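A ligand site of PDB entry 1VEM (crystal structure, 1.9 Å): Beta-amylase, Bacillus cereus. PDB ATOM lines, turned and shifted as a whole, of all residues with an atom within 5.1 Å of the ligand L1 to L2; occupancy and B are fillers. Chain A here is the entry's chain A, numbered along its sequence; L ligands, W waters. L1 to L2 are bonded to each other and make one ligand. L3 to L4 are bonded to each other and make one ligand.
The side-chain hydroxyl of Thr 330 lies within hydrogen-bond range of an oxygen (O2) of LG4 L4, at 2.6 Å.
NH2 of Arg 397 is in hydrogen-bond range of O4 of LG2 L2 (3.0 Å).
O1 of LIG L1 is in hydrogen-bond range of O of Thr 330 (2.7 Å).
An oxygen (O2) of LIG L1 lies within hydrogen-bond range of the backbone carbonyl oxygen (O) of Ala 369, 3.3 Å away.
The side-chain carboxylate of Asp 97 sits at hydrogen-bond distance from an oxygen (O1) of LG2 L2 (2.6 Å).
An oxygen (O5) of LIG L1 lies close to the side-chain hydroxyl (OG1) of Thr 330 (3.5 Å).
The side-chain carboxylate (OD2) of Asp 49 is in hydrogen-bond range of an oxygen (O3) of LG2 L2 (2.5 Å).
An oxygen (O6) of LIG L1 lies within hydrogen-bond range of the side-chain carboxylate (OE1) of Glu 367.
The backbone carbonyl oxygen (O) of Thr 330 lies within hydrogen-bond range of an oxygen (O2) of LG4 L4 (3.4 Å).
An oxygen (O6) of LIG L1 lies within hydrogen-bond range of the side-chain amino group (NZ) of Lys 287 (2.8 Å).
OE1 of Glu 172 is in hydrogen-bond range of O5 of LG4 L4.
O1 of LIG L1 is in hydrogen-bond range of O of Asn 368, at 3.1 Å.
An oxygen (O2) of LG2 L2 sits at hydrogen-bond distance from a ring nitrogen (NE2) of His 89 (2.9 Å).
O of Val 95 sits at hydrogen-bond distance from O3 of LIG L1 (3.4 Å).
An oxygen (O3) of LG4 L4 lies within hydrogen-bond range of an oxygen (O5) of LIG L1 (2.7 Å).
The indole nitrogen of Trp 51 sits at hydrogen-bond distance from the backbone carbonyl oxygen of Leu 19, 3.2 Å away.
The backbone carbonyl oxygen (O) of Glu 367 is in hydrogen-bond range of the backbone NH (N) of Cys 331 (3.3 Å).
The backbone carbonyl oxygen of Leu 396 sits at hydrogen-bond distance from the side-chain amide nitrogen of Asn 368, 2.9 Å away.
The backbone NH (N) of Asn 94 lies within hydrogen-bond range of the side-chain carboxylate (OD2) of Asp 97 (3.1 Å).
The backbone carbonyl oxygen (O) of Ala 17 is in hydrogen-bond range of the guanidinium group (NH1) of Arg 397 (3.1 Å).
NZ of Lys 287 is in salt-bridge range of OE2 of Glu 367, 2.9 Å away.
The guanidinium group (NH1) of Arg 397 is in hydrogen-bond range of the side-chain sulfur (SD) of Met 16.
A ring nitrogen (NE2) of His 89 is in hydrogen-bond range of the backbone NH (N) of Gly 171 (3.3 Å).
OE2 of Glu 172 lies close to O5 of LIG L1, 3.2 Å away.
CE of Met 16 touches O6 of LIG L1, 3.9 Å away.
CD2 of Leu 19 touches O5 of LG2 L2, at 3.8 Å.
CH2 of Trp 51 touches O2 of LG2 L2 (3.4 Å).
Asn 94 touches the ligand L1 to L2.
Ala 170 touches the ligand L1 to L2.
Leu 396 touches the ligand L1 to L2.
Hydrophobic or aromatic side chains that line the ligand L1 to L2: Met 16, Leu 19, Trp 51, His 89, Ala 170, Ala 369 and Leu 396.
17 residues have an atom within 4 Å of the ligand L1 to L2: Met 16, Leu 19, Asp 49, Trp 51, His 89, Asn 94, Val 95, Asp 97, Ala 170, Glu 172, Lys 287, Thr 330, Glu 367, Asn 368, Ala 369, Leu 396 and Arg 397.
Water W2 lies within hydrogen-bond range of O3 of LIG L1 (2.8 Å) and O of Val 95 (2.9 Å).
Water W1 lies within hydrogen-bond range of the side-chain amino group (NZ) of Lys 287 (2.9 Å), an oxygen (O3) of LG2 L2 (3.0 Å) and the backbone carbonyl oxygen (O) of Ala 170 (3.5 Å).
Water W3 lies within hydrogen-bond range of O of Val 95, O3 of LIG L1, OD1 of Asp 97 and NH2 of Arg 397.
Water W6 lies within hydrogen-bond range of O of Ala 369 (2.9 Å), O3 of LIG L1 (3.0 Å) and O of Val 95 (3.4 Å).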
ATOM      1  N   MET A  16      15.413 -36.933   9.666  1.00  0.00           N
ATOM      2  CA  MET A  16      15.634 -36.792  11.109  1.00  0.00           C
ATOM      3  C   MET A  16      14.517 -37.483  11.871  1.00  0.00           C
ATOM      4  O   MET A  16      13.329 -37.322  11.552  1.00  0.00           O
ATOM      5  CB  MET A  16      15.654 -35.330  11.523  1.00  0.00           C
ATOM      6  CG  MET A  16      16.967 -34.628  11.295  1.00  0.00           C
ATOM      7  SD  MET A  16      16.925 -33.039  12.106  1.00  0.00           S
ATOM      8  CE  MET A  16      18.220 -32.167  11.216  1.00  0.00           C
ATOM      9  N   ALA A  17      14.893 -38.244  12.891  1.00  0.00           N
ATOM     10  CA  ALA A  17      13.902 -38.938  13.721  1.00  0.00           C
ATOM     11  C   ALA A  17      13.340 -37.916  14.695  1.00  0.00           C
ATOM     12  O   ALA A  17      13.805 -36.788  14.770  1.00  0.00           O
ATOM     13  CB  ALA A  17      14.581 -40.064  14.480  1.00  0.00           C
ATOM     14  N   LEU A  19      12.608 -36.018  18.288  1.00  0.00           N
ATOM     15  CA  LEU A  19      13.537 -35.719  19.372  1.00  0.00           C
ATOM     16  C   LEU A  19      13.264 -36.663  20.553  1.00  0.00           C
ATOM     17  O   LEU A  19      14.174 -37.011  21.308  1.00  0.00           O
ATOM     18  CB  LEU A  19      13.397 -34.258  19.807  1.00  0.00           C
ATOM     19  CG  LEU A  19      13.874 -33.196  18.811  1.00  0.00           C
ATOM     20  CD1 LEU A  19      13.529 -31.805  19.330  1.00  0.00           C
ATOM     21  CD2 LEU A  19      15.390 -33.315  18.596  1.00  0.00           C
ATOM     22  N   ASP A  49      19.065 -38.797  17.546  1.00  0.00           N
ATOM     23  CA  ASP A  49      19.793 -38.353  18.717  1.00  0.00           C
ATOM     24  C   ASP A  49      19.743 -39.407  19.810  1.00  0.00           C
ATOM     25  O   ASP A  49      18.669 -39.893  20.169  1.00  0.00           O
ATOM     26  CB  ASP A  49      19.168 -37.089  19.337  1.00  0.00           C
ATOM     27  CG  ASP A  49      19.268 -35.878  18.440  1.00  0.00           C
ATOM     28  OD1 ASP A  49      18.359 -35.687  17.601  1.00  0.00           O
ATOM     29  OD2 ASP A  49      20.237 -35.111  18.588  1.00  0.00           O
ATOM     30  N   TRP A  51      20.656 -39.318  23.456  1.00  0.00           N
ATOM     31  CA  TRP A  51      21.005 -38.346  24.486  1.00  0.00           C
ATOM     32  C   TRP A  51      21.901 -38.841  25.601  1.00  0.00           C
ATOM     33  O   TRP A  51      21.652 -39.885  26.210  1.00  0.00           O
ATOM     34  CB  TRP A  51      19.722 -37.768  25.095  1.00  0.00           C
ATOM     35  CG  TRP A  51      18.781 -37.241  24.063  1.00  0.00           C
ATOM     36  CD1 TRP A  51      17.647 -37.841  23.595  1.00  0.00           C
ATOM     37  CD2 TRP A  51      18.927 -36.035  23.301  1.00  0.00           C
ATOM     38  NE1 TRP A  51      17.086 -37.083  22.597  1.00  0.00           N
ATOM     39  CE2 TRP A  51      17.849 -35.965  22.392  1.00  0.00           C
ATOM     40  CE3 TRP A  51      19.880 -34.996  23.300  1.00  0.00           C
ATOM     41  CZ2 TRP A  51      17.694 -34.910  21.488  1.00  0.00           C
ATOM     42  CZ3 TRP A  51      19.720 -33.937  22.404  1.00  0.00           C
ATOM     43  CH2 TRP A  51      18.636 -33.906  21.508  1.00  0.00           C
ATOM     44  N   ILE A  85      23.574 -39.827  16.382  1.00  0.00           N
ATOM     45  CA  ILE A  85      24.175 -38.580  16.808  1.00  0.00           C
ATOM     46  C   ILE A  85      24.452 -38.845  18.280  1.00  0.00           C
ATOM     47  O   ILE A  85      23.538 -39.172  19.025  1.00  0.00           O
ATOM     48  CB  ILE A  85      23.194 -37.396  16.715  1.00  0.00           C
ATOM     49  CG1 ILE A  85      22.669 -37.225  15.288  1.00  0.00           C
ATOM     50  CG2 ILE A  85      23.895 -36.124  17.185  1.00  0.00           C
ATOM     51  CD1 ILE A  85      21.558 -36.207  15.141  1.00  0.00           C
ATOM     52  N   SER A  87      24.575 -37.317  21.109  1.00  0.00           N
ATOM     53  CA  SER A  87      24.186 -36.017  21.640  1.00  0.00           C
ATOM     54  C   SER A  87      24.582 -35.694  23.073  1.00  0.00           C
ATOM     55  O   SER A  87      23.835 -35.949  24.024  1.00  0.00           O
ATOM     56  CB  SER A  87      22.680 -35.844  21.444  1.00  0.00           C
ATOM     57  OG  SER A  87      22.366 -35.907  20.064  1.00  0.00           O
ATOM     58  N   HIS A  89      24.693 -32.908  24.304  1.00  0.00           N
ATOM     59  CA  HIS A  89      24.109 -31.607  24.608  1.00  0.00           C
ATOM     60  C   HIS A  89      22.693 -31.810  25.107  1.00  0.00           C
ATOM     61  O   HIS A  89      22.106 -32.883  24.958  1.00  0.00           O
ATOM     62  CB  HIS A  89      24.092 -30.705  23.369  1.00  0.00           C
ATOM     63  CG  HIS A  89      23.326 -31.263  22.209  1.00  0.00           C
ATOM     64  ND1 HIS A  89      23.836 -32.229  21.378  1.00  0.00           N
ATOM     65  CD2 HIS A  89      22.072 -31.001  21.769  1.00  0.00           C
ATOM     66  CE1 HIS A  89      22.933 -32.541  20.458  1.00  0.00           C
ATOM     67  NE2 HIS A  89      21.848 -31.813  20.685  1.00  0.00           N
ATOM     68  N   GLN A  90      22.120 -30.756  25.691  1.00  0.00           N
ATOM     69  CA  GLN A  90      20.774 -30.815  26.233  1.00  0.00           C
ATOM     70  C   GLN A  90      19.687 -30.694  25.169  1.00  0.00           C
ATOM     71  O   GLN A  90      19.814 -29.902  24.230  1.00  0.00           O
ATOM     72  CB  GLN A  90      20.609 -29.696  27.253  1.00  0.00           C
ATOM     73  CG  GLN A  90      19.176 -29.429  27.684  1.00  0.00           C
ATOM     74  CD  GLN A  90      19.098 -28.238  28.615  1.00  0.00           C
ATOM     75  OE1 GLN A  90      19.649 -28.259  29.723  1.00  0.00           O
ATOM     76  NE2 GLN A  90      18.413 -27.182  28.180  1.00  0.00           N
ATOM     77  N   CYS A  91      18.628 -31.486  25.305  1.00  0.00           N
ATOM     78  CA  CYS A  91      17.501 -31.411  24.381  1.00  0.00           C
ATOM     79  C   CYS A  91      16.486 -30.506  25.083  1.00  0.00           C
ATOM     80  O   CYS A  91      16.131 -30.752  26.242  1.00  0.00           O
ATOM     81  CB  CYS A  91      16.848 -32.787  24.155  1.00  0.00           C
ATOM     82  SG  CYS A  91      15.729 -32.841  22.709  1.00  0.00           S
ATOM     83  N   ASN A  94      16.077 -25.050  22.573  1.00  0.00           N
ATOM     84  CA  ASN A  94      16.440 -24.577  21.248  1.00  0.00           C
ATOM     85  C   ASN A  94      15.255 -24.660  20.292  1.00  0.00           C
ATOM     86  O   ASN A  94      14.309 -25.410  20.533  1.00  0.00           O
ATOM     87  CB  ASN A  94      17.635 -25.378  20.723  1.00  0.00           C
ATOM     88  CG  ASN A  94      18.919 -25.066  21.466  1.00  0.00           C
ATOM     89  OD1 ASN A  94      19.621 -25.963  21.922  1.00  0.00           O
ATOM     90  ND2 ASN A  94      19.232 -23.774  21.600  1.00  0.00           N
ATOM     91  N   VAL A  95      15.304 -23.883  19.221  1.00  0.00           N
ATOM     92  CA  VAL A  95      14.237 -23.832  18.230  1.00  0.00           C
ATOM     93  C   VAL A  95      13.765 -25.208  17.778  1.00  0.00           C
ATOM     94  O   VAL A  95      14.552 -26.045  17.347  1.00  0.00           O
ATOM     95  CB  VAL A  95      14.658 -22.988  16.986  1.00  0.00           C
ATOM     96  CG1 VAL A  95      15.838 -23.642  16.278  1.00  0.00           C
ATOM     97  CG2 VAL A  95      13.471 -22.819  16.041  1.00  0.00           C
ATOM     98  N   ASP A  97      12.675 -27.615  19.602  1.00  0.00           N
ATOM     99  CA  ASP A  97      12.784 -28.631  20.634  1.00  0.00           C
ATOM    100  C   ASP A  97      11.467 -28.930  21.354  1.00  0.00           C
ATOM    101  O   ASP A  97      10.786 -28.038  21.834  1.00  0.00           O
ATOM    102  CB  ASP A  97      13.833 -28.232  21.684  1.00  0.00           C
ATOM    103  CG  ASP A  97      15.258 -28.367  21.186  1.00  0.00           C
ATOM    104  OD1 ASP A  97      15.464 -28.709  20.002  1.00  0.00           O
ATOM    105  OD2 ASP A  97      16.194 -28.132  21.986  1.00  0.00           O
ATOM    106  N   ALA A 170      22.628 -27.655  20.689  1.00  0.00           N
ATOM    107  CA  ALA A 170      21.845 -28.158  19.559  1.00  0.00           C
ATOM    108  C   ALA A 170      22.673 -29.081  18.667  1.00  0.00           C
ATOM    109  O   ALA A 170      22.318 -29.316  17.510  1.00  0.00           O
ATOM    110  CB  ALA A 170      21.300 -26.995  18.739  1.00  0.00           C
ATOM    111  N   GLY A 171      23.775 -29.593  19.205  1.00  0.00           N
ATOM    112  CA  GLY A 171      24.638 -30.486  18.441  1.00  0.00           C
ATOM    113  C   GLY A 171      25.509 -29.769  17.428  1.00  0.00           C
ATOM    114  O   GLY A 171      26.069 -30.387  16.528  1.00  0.00           O
ATOM    115  N   GLU A 172      25.624 -28.453  17.578  1.00  0.00           N
ATOM    116  CA  GLU A 172      26.433 -27.654  16.657  1.00  0.00           C
ATOM    117  C   GLU A 172      27.690 -27.119  17.324  1.00  0.00           C
ATOM    118  O   GLU A 172      27.676 -26.772  18.514  1.00  0.00           O
ATOM    119  CB  GLU A 172      25.585 -26.504  16.097  1.00  0.00           C
ATOM    120  CG  GLU A 172      24.333 -26.975  15.372  1.00  0.00           C
ATOM    121  CD  GLU A 172      23.312 -25.873  15.157  1.00  0.00           C
ATOM    122  OE1 GLU A 172      23.106 -25.059  16.079  1.00  0.00           O
ATOM    123  OE2 GLU A 172      22.706 -25.828  14.070  1.00  0.00           O
ATOM    124  N   LYS A 287      28.531 -30.659  13.059  1.00  0.00           N
ATOM    125  CA  LYS A 287      27.711 -29.616  12.448  1.00  0.00           C
ATOM    126  C   LYS A 287      28.096 -28.183  12.794  1.00  0.00           C
ATOM    127  O   LYS A 287      28.579 -27.900  13.883  1.00  0.00           O
ATOM    128  CB  LYS A 287      26.244 -29.820  12.836  1.00  0.00           C
ATOM    129  CG  LYS A 287      25.716 -31.236  12.645  1.00  0.00           C
ATOM    130  CD  LYS A 287      24.238 -31.296  13.032  1.00  0.00           C
ATOM    131  CE  LYS A 287      23.660 -32.695  12.832  1.00  0.00           C
ATOM    132  NZ  LYS A 287      22.205 -32.712  13.143  1.00  0.00           N
ATOM    133  N   THR A 330      23.668 -26.599   8.771  1.00  0.00           N
ATOM    134  CA  THR A 330      22.262 -26.742   9.145  1.00  0.00           C
ATOM    135  C   THR A 330      21.178 -25.728   8.726  1.00  0.00           C
ATOM    136  O   THR A 330      20.154 -25.637   9.396  1.00  0.00           O
ATOM    137  CB  THR A 330      22.172 -26.932  10.690  1.00  0.00           C
ATOM    138  OG1 THR A 330      22.507 -25.698  11.337  1.00  0.00           O
ATOM    139  CG2 THR A 330      23.152 -27.996  11.156  1.00  0.00           C
ATOM    140  N   CYS A 331      21.386 -24.993   7.636  1.00  0.00           N
ATOM    141  CA  CYS A 331      20.380 -24.023   7.192  1.00  0.00           C
ATOM    142  C   CYS A 331      20.490 -23.736   5.692  1.00  0.00           C
ATOM    143  O   CYS A 331      21.228 -22.840   5.283  1.00  0.00           O
ATOM    144  CB  CYS A 331      20.505 -22.709   7.970  1.00  0.00           C
ATOM    145  SG  CYS A 331      19.201 -21.492   7.619  1.00  0.00           S
ATOM    146  N   GLU A 367      21.185 -29.368   5.858  1.00  0.00           N
ATOM    147  CA  GLU A 367      19.886 -29.601   6.503  1.00  0.00           C
ATOM    148  C   GLU A 367      19.060 -28.333   6.355  1.00  0.00           C
ATOM    149  O   GLU A 367      19.592 -27.268   6.034  1.00  0.00           O
ATOM    150  CB  GLU A 367      20.035 -29.854   8.010  1.00  0.00           C
ATOM    151  CG  GLU A 367      21.148 -30.777   8.458  1.00  0.00           C
ATOM    152  CD  GLU A 367      21.134 -30.990   9.970  1.00  0.00           C
ATOM    153  OE1 GLU A 367      20.767 -30.048  10.720  1.00  0.00           O
ATOM    154  OE2 GLU A 367      21.487 -32.094  10.412  1.00  0.00           O
ATOM    155  N   ASN A 368      17.762 -28.454   6.587  1.00  0.00           N
ATOM    156  CA  ASN A 368      16.895 -27.279   6.559  1.00  0.00           C
ATOM    157  C   ASN A 368      16.849 -26.858   8.040  1.00  0.00           C
ATOM    158  O   ASN A 368      16.875 -27.706   8.927  1.00  0.00           O
ATOM    159  CB  ASN A 368      15.490 -27.614   6.035  1.00  0.00           C
ATOM    160  CG  ASN A 368      14.861 -28.813   6.738  1.00  0.00           C
ATOM    161  OD1 ASN A 368      15.386 -29.929   6.679  1.00  0.00           O
ATOM    162  ND2 ASN A 368      13.725 -28.585   7.392  1.00  0.00           N
ATOM    163  N   ALA A 369      16.822 -25.547   8.294  1.00  0.00           N
ATOM    164  CA  ALA A 369      16.793 -25.043   9.668  1.00  0.00           C
ATOM    165  C   ALA A 369      15.432 -25.181  10.352  1.00  0.00           C
ATOM    166  O   ALA A 369      15.361 -25.563  11.525  1.00  0.00           O
ATOM    167  CB  ALA A 369      17.235 -23.582   9.688  1.00  0.00           C
ATOM    168  N   LEU A 396      14.564 -32.142   8.334  1.00  0.00           N
ATOM    169  CA  LEU A 396      14.029 -31.997   9.667  1.00  0.00           C
ATOM    170  C   LEU A 396      12.549 -31.663   9.400  1.00  0.00           C
ATOM    171  O   LEU A 396      12.265 -30.696   8.700  1.00  0.00           O
ATOM    172  CB  LEU A 396      14.730 -30.816  10.364  1.00  0.00           C
ATOM    173  CG  LEU A 396      14.292 -30.319  11.748  1.00  0.00           C
ATOM    174  CD1 LEU A 396      15.406 -29.424  12.310  1.00  0.00           C
ATOM    175  CD2 LEU A 396      12.969 -29.558  11.656  1.00  0.00           C
ATOM    176  N   ARG A 397      11.599 -32.450   9.918  1.00  0.00           N
ATOM    177  CA  ARG A 397      11.855 -33.625  10.730  1.00  0.00           C
ATOM    178  C   ARG A 397      10.740 -34.643  10.442  1.00  0.00           C
ATOM    179  O   ARG A 397       9.709 -34.307   9.854  1.00  0.00           O
ATOM    180  CB  ARG A 397      11.835 -33.235  12.212  1.00  0.00           C
ATOM    181  CG  ARG A 397      12.259 -34.338  13.172  1.00  0.00           C
ATOM    182  CD  ARG A 397      12.139 -33.864  14.617  1.00  0.00           C
ATOM    183  NE  ARG A 397      12.983 -32.702  14.894  1.00  0.00           N
ATOM    184  CZ  ARG A 397      14.298 -32.770  15.091  1.00  0.00           C
ATOM    185  NH1 ARG A 397      14.927 -33.932  15.057  1.00  0.00           N
ATOM    186  NH2 ARG A 397      14.977 -31.656  15.358  1.00  0.00           N
HETATM  187  C1  LIG L   1      18.998 -27.899  12.447  1.00  0.00           C
HETATM  188  C2  LIG L   1      17.939 -26.984  13.109  1.00  0.00           C
HETATM  189  C3  LIG L   1      17.950 -27.263  14.612  1.00  0.00           C
HETATM  190  C4  LIG L   1      18.832 -28.491  14.859  1.00  0.00           C
HETATM  191  C5  LIG L   1      20.266 -28.199  14.408  1.00  0.00           C
HETATM  192  C6  LIG L   1      21.130 -29.438  14.375  1.00  0.00           C
HETATM  193  O1  LIG L   1      19.121 -27.510  11.120  1.00  0.00           O
HETATM  194  O2  LIG L   1      18.327 -25.655  12.874  1.00  0.00           O
HETATM  195  O3  LIG L   1      16.628 -27.527  15.089  1.00  0.00           O
HETATM  196  O4  LIG L   1      18.792 -28.860  16.236  1.00  0.00           O
HETATM  197  O5  LIG L   1      20.240 -27.666  13.089  1.00  0.00           O
HETATM  198  O6  LIG L   1      20.892 -30.283  13.261  1.00  0.00           O
HETATM  199  C1  LG2 L   2      17.786 -29.779  16.617  1.00  0.00           C
HETATM  200  C2  LG2 L   2      17.817 -29.998  18.131  1.00  0.00           C
HETATM  201  C3  LG2 L   2      19.127 -30.718  18.489  1.00  0.00           C
HETATM  202  C4  LG2 L   2      19.179 -32.068  17.760  1.00  0.00           C
HETATM  203  C5  LG2 L   2      19.068 -31.830  16.243  1.00  0.00           C
HETATM  204  C6  LG2 L   2      19.003 -33.114  15.402  1.00  0.00           C
HETATM  205  O1  LG2 L   2      17.765 -28.736  18.786  1.00  0.00           O
HETATM  206  O2  LG2 L   2      19.217 -30.924  19.898  1.00  0.00           O
HETATM  207  O3  LG2 L   2      20.422 -32.708  18.063  1.00  0.00           O
HETATM  208  O4  LG2 L   2      17.876 -31.048  15.938  1.00  0.00           O
HETATM  209  O5  LG2 L   2      17.889 -33.946  15.740  1.00  0.00           O
HETATM  210  C1  LG3 L   3      14.877 -18.341  13.865  1.00  0.00           C
HETATM  211  C2  LG3 L   3      15.600 -18.419  12.512  1.00  0.00           C
HETATM  212  C3  LG3 L   3      16.435 -19.699  12.430  1.00  0.00           C
HETATM  213  C4  LG3 L   3      17.386 -19.789  13.625  1.00  0.00           C
HETATM  214  C5  LG3 L   3      16.587 -19.659  14.929  1.00  0.00           C
HETATM  215  C6  LG3 L   3      17.498 -19.611  16.146  1.00  0.00           C
HETATM  216  O1  LG3 L   3      13.998 -19.408  13.987  1.00  0.00           O
HETATM  217  O2  LG3 L   3      14.668 -18.399  11.449  1.00  0.00           O
HETATM  218  O3  LG3 L   3      17.180 -19.725  11.236  1.00  0.00           O
HETATM  219  O4  LG3 L   3      18.088 -21.047  13.571  1.00  0.00           O
HETATM  220  O5  LG3 L   3      15.814 -18.435  14.946  1.00  0.00           O
HETATM  221  O6  LG3 L   3      16.774 -19.808  17.351  1.00  0.00           O
HETATM  222  C1  LG4 L   4      19.451 -20.976  13.921  1.00  0.00           C
HETATM  223  C2  LG4 L   4      20.325 -21.436  12.746  1.00  0.00           C
HETATM  224  C3  LG4 L   4      20.313 -22.975  12.593  1.00  0.00           C
HETATM  225  C4  LG4 L   4      20.531 -23.684  13.939  1.00  0.00           C
HETATM  226  C5  LG4 L   4      19.576 -23.139  14.990  1.00  0.00           C
HETATM  227  C6  LG4 L   4      19.860 -23.739  16.353  1.00  0.00           C
HETATM  228  O1  LG4 L   4      19.853 -20.834  11.544  1.00  0.00           O
HETATM  229  O2  LG4 L   4      21.339 -23.366  11.702  1.00  0.00           O
HETATM  230  O3  LG4 L   4      20.304 -25.077  13.782  1.00  0.00           O
HETATM  231  O4  LG4 L   4      19.749 -21.722  15.108  1.00  0.00           O
HETATM  232  O5  LG4 L   4      21.226 -23.550  16.708  1.00  0.00           O
HETATM  233  O   HOH W   1      22.559 -32.405  15.986  1.00  0.00           O
HETATM  234  O   HOH W   2      17.440 -26.201  17.384  1.00  0.00           O
HETATM  235  O   HOH W   3      14.557 -28.762  16.932  1.00  0.00           O
HETATM  236  O   HOH W   4      18.809 -28.769  21.722  1.00  0.00           O
HETATM  237  O   HOH W   5      17.813 -36.416  14.108  1.00  0.00           O
HETATM  238  O   HOH W   6      14.019 -26.383  14.012  1.00  0.00           O
